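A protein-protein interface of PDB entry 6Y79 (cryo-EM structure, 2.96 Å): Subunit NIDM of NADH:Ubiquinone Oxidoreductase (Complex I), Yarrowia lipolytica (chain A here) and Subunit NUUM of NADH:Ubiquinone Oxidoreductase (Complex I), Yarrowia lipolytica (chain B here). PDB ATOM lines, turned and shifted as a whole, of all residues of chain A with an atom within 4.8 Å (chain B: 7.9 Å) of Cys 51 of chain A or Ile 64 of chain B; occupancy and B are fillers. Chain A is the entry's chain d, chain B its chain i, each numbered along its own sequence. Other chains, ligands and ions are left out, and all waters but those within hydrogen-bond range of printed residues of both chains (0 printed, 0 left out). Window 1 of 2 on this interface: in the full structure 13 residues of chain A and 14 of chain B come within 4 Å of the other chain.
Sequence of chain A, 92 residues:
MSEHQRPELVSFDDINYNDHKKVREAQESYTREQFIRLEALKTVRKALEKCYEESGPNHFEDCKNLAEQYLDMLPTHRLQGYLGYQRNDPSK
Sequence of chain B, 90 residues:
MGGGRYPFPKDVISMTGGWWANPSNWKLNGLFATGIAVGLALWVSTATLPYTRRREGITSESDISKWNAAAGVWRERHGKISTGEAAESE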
ATOM      1  N   ALA A  47       9.881  13.455  -6.356  1.00  0.00           N
ATOM      2  CA  ALA A  47       9.313  14.797  -6.254  1.00  0.00           C
ATOM      3  C   ALA A  47       8.385  14.922  -5.052  1.00  0.00           C
ATOM      4  O   ALA A  47       8.372  15.953  -4.372  1.00  0.00           O
ATOM      5  CB  ALA A  47       8.561  15.141  -7.537  1.00  0.00           C
ATOM      6  N   LEU A  48       7.629  13.866  -4.755  1.00  0.00           N
ATOM      7  CA  LEU A  48       6.707  13.901  -3.626  1.00  0.00           C
ATOM      8  C   LEU A  48       7.446  13.901  -2.297  1.00  0.00           C
ATOM      9  O   LEU A  48       7.039  14.594  -1.358  1.00  0.00           O
ATOM     10  CB  LEU A  48       5.756  12.715  -3.703  1.00  0.00           C
ATOM     11  CG  LEU A  48       4.870  12.416  -2.502  1.00  0.00           C
ATOM     12  CD1 LEU A  48       3.901  13.548  -2.238  1.00  0.00           C
ATOM     13  CD2 LEU A  48       4.141  11.137  -2.775  1.00  0.00           C
ATOM     14  N   GLU A  49       8.528  13.132  -2.182  1.00  0.00           N
ATOM     15  CA  GLU A  49       9.246  13.145  -0.912  1.00  0.00           C
ATOM     16  C   GLU A  49      10.069  14.416  -0.759  1.00  0.00           C
ATOM     17  O   GLU A  49      10.306  14.868   0.365  1.00  0.00           O
ATOM     18  CB  GLU A  49      10.112  11.901  -0.746  1.00  0.00           C
ATOM     19  CG  GLU A  49      11.277  11.768  -1.672  1.00  0.00           C
ATOM     20  CD  GLU A  49      12.017  10.471  -1.432  1.00  0.00           C
ATOM     21  OE1 GLU A  49      11.594   9.702  -0.539  1.00  0.00           O
ATOM     22  OE2 GLU A  49      13.014  10.214  -2.138  1.00  0.00           O
ATOM     23  N   LYS A  50      10.460  15.046  -1.871  1.00  0.00           N
ATOM     24  CA  LYS A  50      10.993  16.401  -1.777  1.00  0.00           C
ATOM     25  C   LYS A  50       9.933  17.386  -1.296  1.00  0.00           C
ATOM     26  O   LYS A  50      10.235  18.261  -0.484  1.00  0.00           O
ATOM     27  CB  LYS A  50      11.563  16.850  -3.116  1.00  0.00           C
ATOM     28  CG  LYS A  50      12.969  16.388  -3.371  1.00  0.00           C
ATOM     29  CD  LYS A  50      13.448  16.921  -4.692  1.00  0.00           C
ATOM     30  CE  LYS A  50      14.846  16.458  -4.983  1.00  0.00           C
ATOM     31  NZ  LYS A  50      15.251  16.871  -6.344  1.00  0.00           N
ATOM     32  N   CYS A  51       8.686  17.242  -1.766  1.00  0.00           N
ATOM     33  CA  CYS A  51       7.588  18.077  -1.266  1.00  0.00           C
ATOM     34  C   CYS A  51       7.373  17.896   0.227  1.00  0.00           C
ATOM     35  O   CYS A  51       7.248  18.874   0.970  1.00  0.00           O
ATOM     36  CB  CYS A  51       6.272  17.762  -1.975  1.00  0.00           C
ATOM     37  SG  CYS A  51       4.892  18.542  -1.062  1.00  0.00           S
ATOM     38  N   TYR A  52       7.322  16.642   0.674  1.00  0.00           N
ATOM     39  CA  TYR A  52       7.088  16.341   2.078  1.00  0.00           C
ATOM     40  C   TYR A  52       8.208  16.851   2.957  1.00  0.00           C
ATOM     41  O   TYR A  52       7.956  17.402   4.029  1.00  0.00           O
ATOM     42  CB  TYR A  52       6.921  14.843   2.273  1.00  0.00           C
ATOM     43  CG  TYR A  52       6.675  14.445   3.708  1.00  0.00           C
ATOM     44  CD1 TYR A  52       5.430  14.622   4.277  1.00  0.00           C
ATOM     45  CD2 TYR A  52       7.685  13.890   4.493  1.00  0.00           C
ATOM     46  CE1 TYR A  52       5.181  14.263   5.586  1.00  0.00           C
ATOM     47  CE2 TYR A  52       7.445  13.532   5.804  1.00  0.00           C
ATOM     48  CZ  TYR A  52       6.190  13.721   6.342  1.00  0.00           C
ATOM     49  OH  TYR A  52       5.926  13.372   7.643  1.00  0.00           O
ATOM     50  N   GLU A  53       9.451  16.670   2.531  1.00  0.00           N
ATOM     51  CA  GLU A  53      10.573  17.173   3.318  1.00  0.00           C
ATOM     52  C   GLU A  53      10.654  18.684   3.298  1.00  0.00           C
ATOM     53  O   GLU A  53      11.030  19.273   4.326  1.00  0.00           O
ATOM     54  CB  GLU A  53      11.864  16.530   2.804  1.00  0.00           C
ATOM     55  CG  GLU A  53      11.982  15.078   3.162  1.00  0.00           C
ATOM     56  CD  GLU A  53      13.259  14.471   2.667  1.00  0.00           C
ATOM     57  OE1 GLU A  53      14.038  15.202   2.033  1.00  0.00           O
ATOM     58  OE2 GLU A  53      13.481  13.265   2.905  1.00  0.00           O
ATOM     59  N   GLU A  54      10.316  19.333   2.172  1.00  0.00           N
ATOM     60  CA  GLU A  54      10.333  20.784   2.216  1.00  0.00           C
ATOM     61  C   GLU A  54       9.118  21.350   2.927  1.00  0.00           C
ATOM     62  O   GLU A  54       9.120  22.524   3.295  1.00  0.00           O
ATOM     63  CB  GLU A  54      10.412  21.358   0.823  1.00  0.00           C
ATOM     64  CG  GLU A  54      11.670  21.072   0.073  1.00  0.00           C
ATOM     65  CD  GLU A  54      12.863  21.747   0.655  1.00  0.00           C
ATOM     66  OE1 GLU A  54      12.774  22.953   0.962  1.00  0.00           O
ATOM     67  OE2 GLU A  54      13.892  21.062   0.821  1.00  0.00           O
ATOM     68  N   SER A  55       8.036  20.590   3.055  1.00  0.00           N
ATOM     69  CA  SER A  55       6.805  21.231   3.500  1.00  0.00           C
ATOM     70  C   SER A  55       6.718  21.274   5.013  1.00  0.00           C
ATOM     71  O   SER A  55       6.343  22.291   5.592  1.00  0.00           O
ATOM     72  CB  SER A  55       5.559  20.529   2.944  1.00  0.00           C
ATOM     73  OG  SER A  55       4.438  21.110   3.623  1.00  0.00           O
ATOM     74  N   ASP A  62      -0.038  21.294   0.505  1.00  0.00           N
ATOM     75  CA  ASP A  62       0.858  21.658  -0.584  1.00  0.00           C
ATOM     76  C   ASP A  62       0.873  20.565  -1.633  1.00  0.00           C
ATOM     77  O   ASP A  62       0.708  20.852  -2.814  1.00  0.00           O
ATOM     78  CB  ASP A  62       2.276  21.942  -0.076  1.00  0.00           C
ATOM     79  CG  ASP A  62       3.182  22.613  -1.144  1.00  0.00           C
ATOM     80  OD1 ASP A  62       3.356  22.110  -2.291  1.00  0.00           O
ATOM     81  OD2 ASP A  62       3.712  23.702  -0.848  1.00  0.00           O
ATOM     82  N   CYS A  63       1.040  19.312  -1.237  1.00  0.00           N
ATOM     83  CA  CYS A  63       1.083  18.240  -2.219  1.00  0.00           C
ATOM     84  C   CYS A  63       0.035  17.184  -1.911  1.00  0.00           C
ATOM     85  O   CYS A  63       0.327  15.999  -1.749  1.00  0.00           O
ATOM     86  CB  CYS A  63       2.480  17.652  -2.375  1.00  0.00           C
ATOM     87  SG  CYS A  63       3.395  17.155  -0.935  1.00  0.00           S
ATOM     88  N   LEU A  66       0.215  15.810  -5.601  1.00  0.00           N
ATOM     89  CA  LEU A  66       1.341  14.906  -5.844  1.00  0.00           C
ATOM     90  C   LEU A  66       1.124  13.552  -5.180  1.00  0.00           C
ATOM     91  O   LEU A  66       1.465  12.510  -5.751  1.00  0.00           O
ATOM     92  CB  LEU A  66       2.644  15.521  -5.344  1.00  0.00           C
ATOM     93  CG  LEU A  66       3.353  16.552  -6.208  1.00  0.00           C
ATOM     94  CD1 LEU A  66       4.579  17.075  -5.490  1.00  0.00           C
ATOM     95  CD2 LEU A  66       3.741  15.940  -7.528  1.00  0.00           C
ATOM     96  N   GLU B  56      15.442  19.924   5.209  1.00  0.00           N
ATOM     97  CA  GLU B  56      14.720  21.107   4.754  1.00  0.00           C
ATOM     98  C   GLU B  56      15.698  22.058   4.070  1.00  0.00           C
ATOM     99  O   GLU B  56      16.846  22.208   4.489  1.00  0.00           O
ATOM    100  CB  GLU B  56      14.039  21.839   5.940  1.00  0.00           C
ATOM    101  CG  GLU B  56      13.382  23.156   5.615  1.00  0.00           C
ATOM    102  CD  GLU B  56      12.050  22.989   4.877  1.00  0.00           C
ATOM    103  OE1 GLU B  56      11.231  22.164   5.339  1.00  0.00           O
ATOM    104  OE2 GLU B  56      11.947  23.587   3.794  1.00  0.00           O
ATOM    105  N   THR B  59      15.383  22.131  -1.905  1.00  0.00           N
ATOM    106  CA  THR B  59      14.786  22.645  -3.126  1.00  0.00           C
ATOM    107  C   THR B  59      13.961  23.888  -2.819  1.00  0.00           C
ATOM    108  O   THR B  59      13.512  24.078  -1.681  1.00  0.00           O
ATOM    109  CB  THR B  59      13.921  21.577  -3.814  1.00  0.00           C
ATOM    110  OG1 THR B  59      12.796  21.249  -2.996  1.00  0.00           O
ATOM    111  CG2 THR B  59      14.737  20.323  -4.046  1.00  0.00           C
ATOM    112  N   SER B  60      13.792  24.740  -3.841  1.00  0.00           N
ATOM    113  CA  SER B  60      12.958  25.923  -3.695  1.00  0.00           C
ATOM    114  C   SER B  60      11.498  25.557  -3.522  1.00  0.00           C
ATOM    115  O   SER B  60      11.057  24.468  -3.895  1.00  0.00           O
ATOM    116  CB  SER B  60      13.093  26.846  -4.874  1.00  0.00           C
ATOM    117  OG  SER B  60      12.602  26.275  -6.049  1.00  0.00           O
ATOM    118  N   GLU B  61      10.733  26.505  -2.975  1.00  0.00           N
ATOM    119  CA  GLU B  61       9.286  26.324  -2.909  1.00  0.00           C
ATOM    120  C   GLU B  61       8.619  26.591  -4.249  1.00  0.00           C
ATOM    121  O   GLU B  61       7.450  26.204  -4.446  1.00  0.00           O
ATOM    122  CB  GLU B  61       8.702  27.213  -1.825  1.00  0.00           C
ATOM    123  CG  GLU B  61       8.715  28.703  -2.096  1.00  0.00           C
ATOM    124  CD  GLU B  61       8.148  29.476  -0.921  1.00  0.00           C
ATOM    125  OE1 GLU B  61       7.795  28.829   0.089  1.00  0.00           O
ATOM    126  OE2 GLU B  61       8.047  30.714  -1.005  1.00  0.00           O
ATOM    127  N   SER B  62       9.339  27.269  -5.163  1.00  0.00           N
ATOM    128  CA  SER B  62       8.889  27.377  -6.544  1.00  0.00           C
ATOM    129  C   SER B  62       8.713  26.004  -7.154  1.00  0.00           C
ATOM    130  O   SER B  62       7.693  25.729  -7.808  1.00  0.00           O
ATOM    131  CB  SER B  62       9.884  28.171  -7.369  1.00  0.00           C
ATOM    132  OG  SER B  62      11.057  27.468  -7.549  1.00  0.00           O
ATOM    133  N   ASP B  63       9.710  25.136  -6.931  1.00  0.00           N
ATOM    134  CA  ASP B  63       9.690  23.756  -7.414  1.00  0.00           C
ATOM    135  C   ASP B  63       8.426  23.018  -6.979  1.00  0.00           C
ATOM    136  O   ASP B  63       7.707  22.462  -7.809  1.00  0.00           O
ATOM    137  CB  ASP B  63      10.910  22.990  -6.899  1.00  0.00           C
ATOM    138  CG  ASP B  63      12.174  23.383  -7.588  1.00  0.00           C
ATOM    139  OD1 ASP B  63      12.164  24.305  -8.441  1.00  0.00           O
ATOM    140  OD2 ASP B  63      13.198  22.733  -7.313  1.00  0.00           O
ATOM    141  N   ILE B  64       8.100  23.056  -5.694  1.00  0.00           N
ATOM    142  CA  ILE B  64       7.023  22.206  -5.196  1.00  0.00           C
ATOM    143  C   ILE B  64       5.659  22.801  -5.532  1.00  0.00           C
ATOM    144  O   ILE B  64       4.675  22.066  -5.721  1.00  0.00           O
ATOM    145  CB  ILE B  64       7.192  21.941  -3.691  1.00  0.00           C
ATOM    146  CG1 ILE B  64       7.156  23.213  -2.865  1.00  0.00           C
ATOM    147  CG2 ILE B  64       8.499  21.178  -3.465  1.00  0.00           C
ATOM    148  CD1 ILE B  64       7.509  23.001  -1.390  1.00  0.00           C
ATOM    149  N   SER B  65       5.588  24.140  -5.659  1.00  0.00           N
ATOM    150  CA  SER B  65       4.365  24.772  -6.157  1.00  0.00           C
ATOM    151  C   SER B  65       4.077  24.382  -7.603  1.00  0.00           C
ATOM    152  O   SER B  65       2.940  24.026  -7.949  1.00  0.00           O
ATOM    153  CB  SER B  65       4.476  26.283  -6.031  1.00  0.00           C
ATOM    154  OG  SER B  65       4.567  26.689  -4.679  1.00  0.00           O
ATOM    155  N   LYS B  66       5.097  24.411  -8.460  1.00  0.00           N
ATOM    156  CA  LYS B  66       4.852  24.027  -9.843  1.00  0.00           C
ATOM    157  C   LYS B  66       4.725  22.516 -10.024  1.00  0.00           C
ATOM    158  O   LYS B  66       4.064  22.078 -10.969  1.00  0.00           O
ATOM    159  CB  LYS B  66       5.936  24.617 -10.743  1.00  0.00           C
ATOM    160  CG  LYS B  66       7.281  23.984 -10.607  1.00  0.00           C
ATOM    161  CD  LYS B  66       8.356  24.883 -11.144  1.00  0.00           C
ATOM    162  CE  LYS B  66       9.642  24.113 -11.332  1.00  0.00           C
ATOM    163  NZ  LYS B  66      10.722  24.977 -11.864  1.00  0.00           N
ATOM    164  N   TRP B  67       5.275  21.707  -9.113  1.00  0.00           N
ATOM    165  CA  TRP B  67       5.034  20.269  -9.177  1.00  0.00           C
ATOM    166  C   TRP B  67       3.615  19.933  -8.747  1.00  0.00           C
ATOM    167  O   TRP B  67       2.995  19.023  -9.303  1.00  0.00           O
ATOM    168  CB  TRP B  67       6.025  19.511  -8.306  1.00  0.00           C
ATOM    169  CG  TRP B  67       7.422  19.572  -8.771  1.00  0.00           C
ATOM    170  CD1 TRP B  67       7.867  19.987  -9.983  1.00  0.00           C
ATOM    171  CD2 TRP B  67       8.581  19.235  -8.011  1.00  0.00           C
ATOM    172  NE1 TRP B  67       9.235  19.919 -10.034  1.00  0.00           N
ATOM    173  CE2 TRP B  67       9.697  19.460  -8.831  1.00  0.00           C
ATOM    174  CE3 TRP B  67       8.783  18.758  -6.715  1.00  0.00           C
ATOM    175  CZ2 TRP B  67      10.995  19.224  -8.399  1.00  0.00           C
ATOM    176  CZ3 TRP B  67      10.069  18.526  -6.290  1.00  0.00           C
ATOM    177  CH2 TRP B  67      11.159  18.758  -7.127  1.00  0.00           C
ATOM    178  N   ASN B  68       3.091  20.652  -7.751  1.00  0.00           N
ATOM    179  CA  ASN B  68       1.678  20.544  -7.408  1.00  0.00           C
ATOM    180  C   ASN B  68       0.791  20.977  -8.571  1.00  0.00           C
ATOM    181  O   ASN B  68      -0.248  20.356  -8.835  1.00  0.00           O
ATOM    182  CB  ASN B  68       1.393  21.399  -6.181  1.00  0.00           C
ATOM    183  CG  ASN B  68      -0.011  21.238  -5.672  1.00  0.00           C
ATOM    184  OD1 ASN B  68      -0.658  20.237  -5.925  1.00  0.00           O
ATOM    185  ND2 ASN B  68      -0.477  22.217  -4.907  1.00  0.00           N
ATOM    186  N   ALA B  69       1.196  22.033  -9.282  1.00  0.00           N
ATOM    187  CA  ALA B  69       0.447  22.485 -10.453  1.00  0.00           C
ATOM    188  C   ALA B  69       0.451  21.431 -11.560  1.00  0.00           C
ATOM    189  O   ALA B  69      -0.592  21.139 -12.159  1.00  0.00           O
ATOM    190  CB  ALA B  69       1.029  23.807 -10.958  1.00  0.00           C
ATOM    191  N   ALA B  70       1.610  20.824 -11.826  1.00  0.00           N
ATOM    192  CA  ALA B  70       1.698  19.786 -12.852  1.00  0.00           C
ATOM    193  C   ALA B  70       1.008  18.498 -12.432  1.00  0.00           C
ATOM    194  O   ALA B  70       0.565  17.725 -13.286  1.00  0.00           O
ATOM    195  CB  ALA B  70       3.153  19.495 -13.194  1.00  0.00           C
ATOM    196  N   ALA B  71       0.919  18.237 -11.132  1.00  0.00           N
ATOM    197  CA  ALA B  71       0.117  17.111 -10.673  1.00  0.00           C
ATOM    198  C   ALA B  71      -1.363  17.388 -10.880  1.00  0.00           C
ATOM    199  O   ALA B  71      -2.126  16.482 -11.220  1.00  0.00           O
ATOM    200  CB  ALA B  71       0.414  16.813  -9.206  1.00  0.00           C
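Of the 14 printed residues of chain B, 6 touch a printed residue of chain A. Hydrophobic or aromatic side chains of chain B that line the printed part of chain A: Ile 64, Trp 67 and Ala 71. Hydrophobic or aromatic side chains of chain A within 4 Å of the printed part of chain B: Ala 47 and Leu 66. Among the printed residues, 11 pairs touch across the chains. Among the printed residues, no Asp or Glu carboxylate lies within 4 Å of a Lys or Arg side-chain nitrogen of the other chain.
Ala 47 of chain A touches Trp 67 of chain B. CD of Lys 50 of chain A touches CG2 of Thr 59 of chain B, at 3.7 Å. Lys 50 of chain A touches Trp 67 of chain B. CA of Cys 51 of chain A touches CG2 of Ile 64 of chain B, at 3.9 Å. OD1 of Asp 62 of chain A touches O of Ile 64 of chain B, 3.7 Å away. Leu 66 of chain A touches Trp 67 of chain B (CD2 to O, 3.6 Å). N of Leu 66 of chain A touches CB of Ala 71 of chain B, 3.7 Å away.
Cys 51 of chain A touches just one residue of chain B: Ile 64. Of the printed residues of chain A, Ile 64 of chain B touches Cys 51 and Asp 62. Printed residues of chain B within 4 Å of Glu 53 of chain A: Glu 56. Of the printed residues of chain B, Leu 66 of chain A touches Trp 67 and Ala 71. Of the printed residues of chain A, Asn 68 of chain B touches Asp 62. Ala 69 of chain B touches none of the printed residues of chain A. Ala 70 of chain B touches none of the printed residues of chain A. The nearest residue of chain B that does not touch Cys 51 of chain A is Trp 67 of chain B (4.9 Å). The nearest printed residue of chain B that does not touch Asp 62 of chain A is Ser 65 of chain B (4.5 Å).
The side-chain carboxylate (OE2) of Glu 54 of chain A sits at hydrogen-bond distance from the backbone NH (N) of Thr 59 of chain B, 3.3 Å away. O of Asp 62 of chain A sits at hydrogen-bond distance from ND2 of Asn 68 of chain B. The backbone carbonyl oxygen (O) of Glu 53 of chain A lies close to the side-chain carboxylate (OE1) of Glu 56 of chain B. OE1 of Glu 56 of chain B lies close to O of Glu 54 of chain A, at 3.0 Å.
SG of Cys 63 of chain A is disulfide-bonded to SG of Cys 51 of chain A (2.0 Å).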
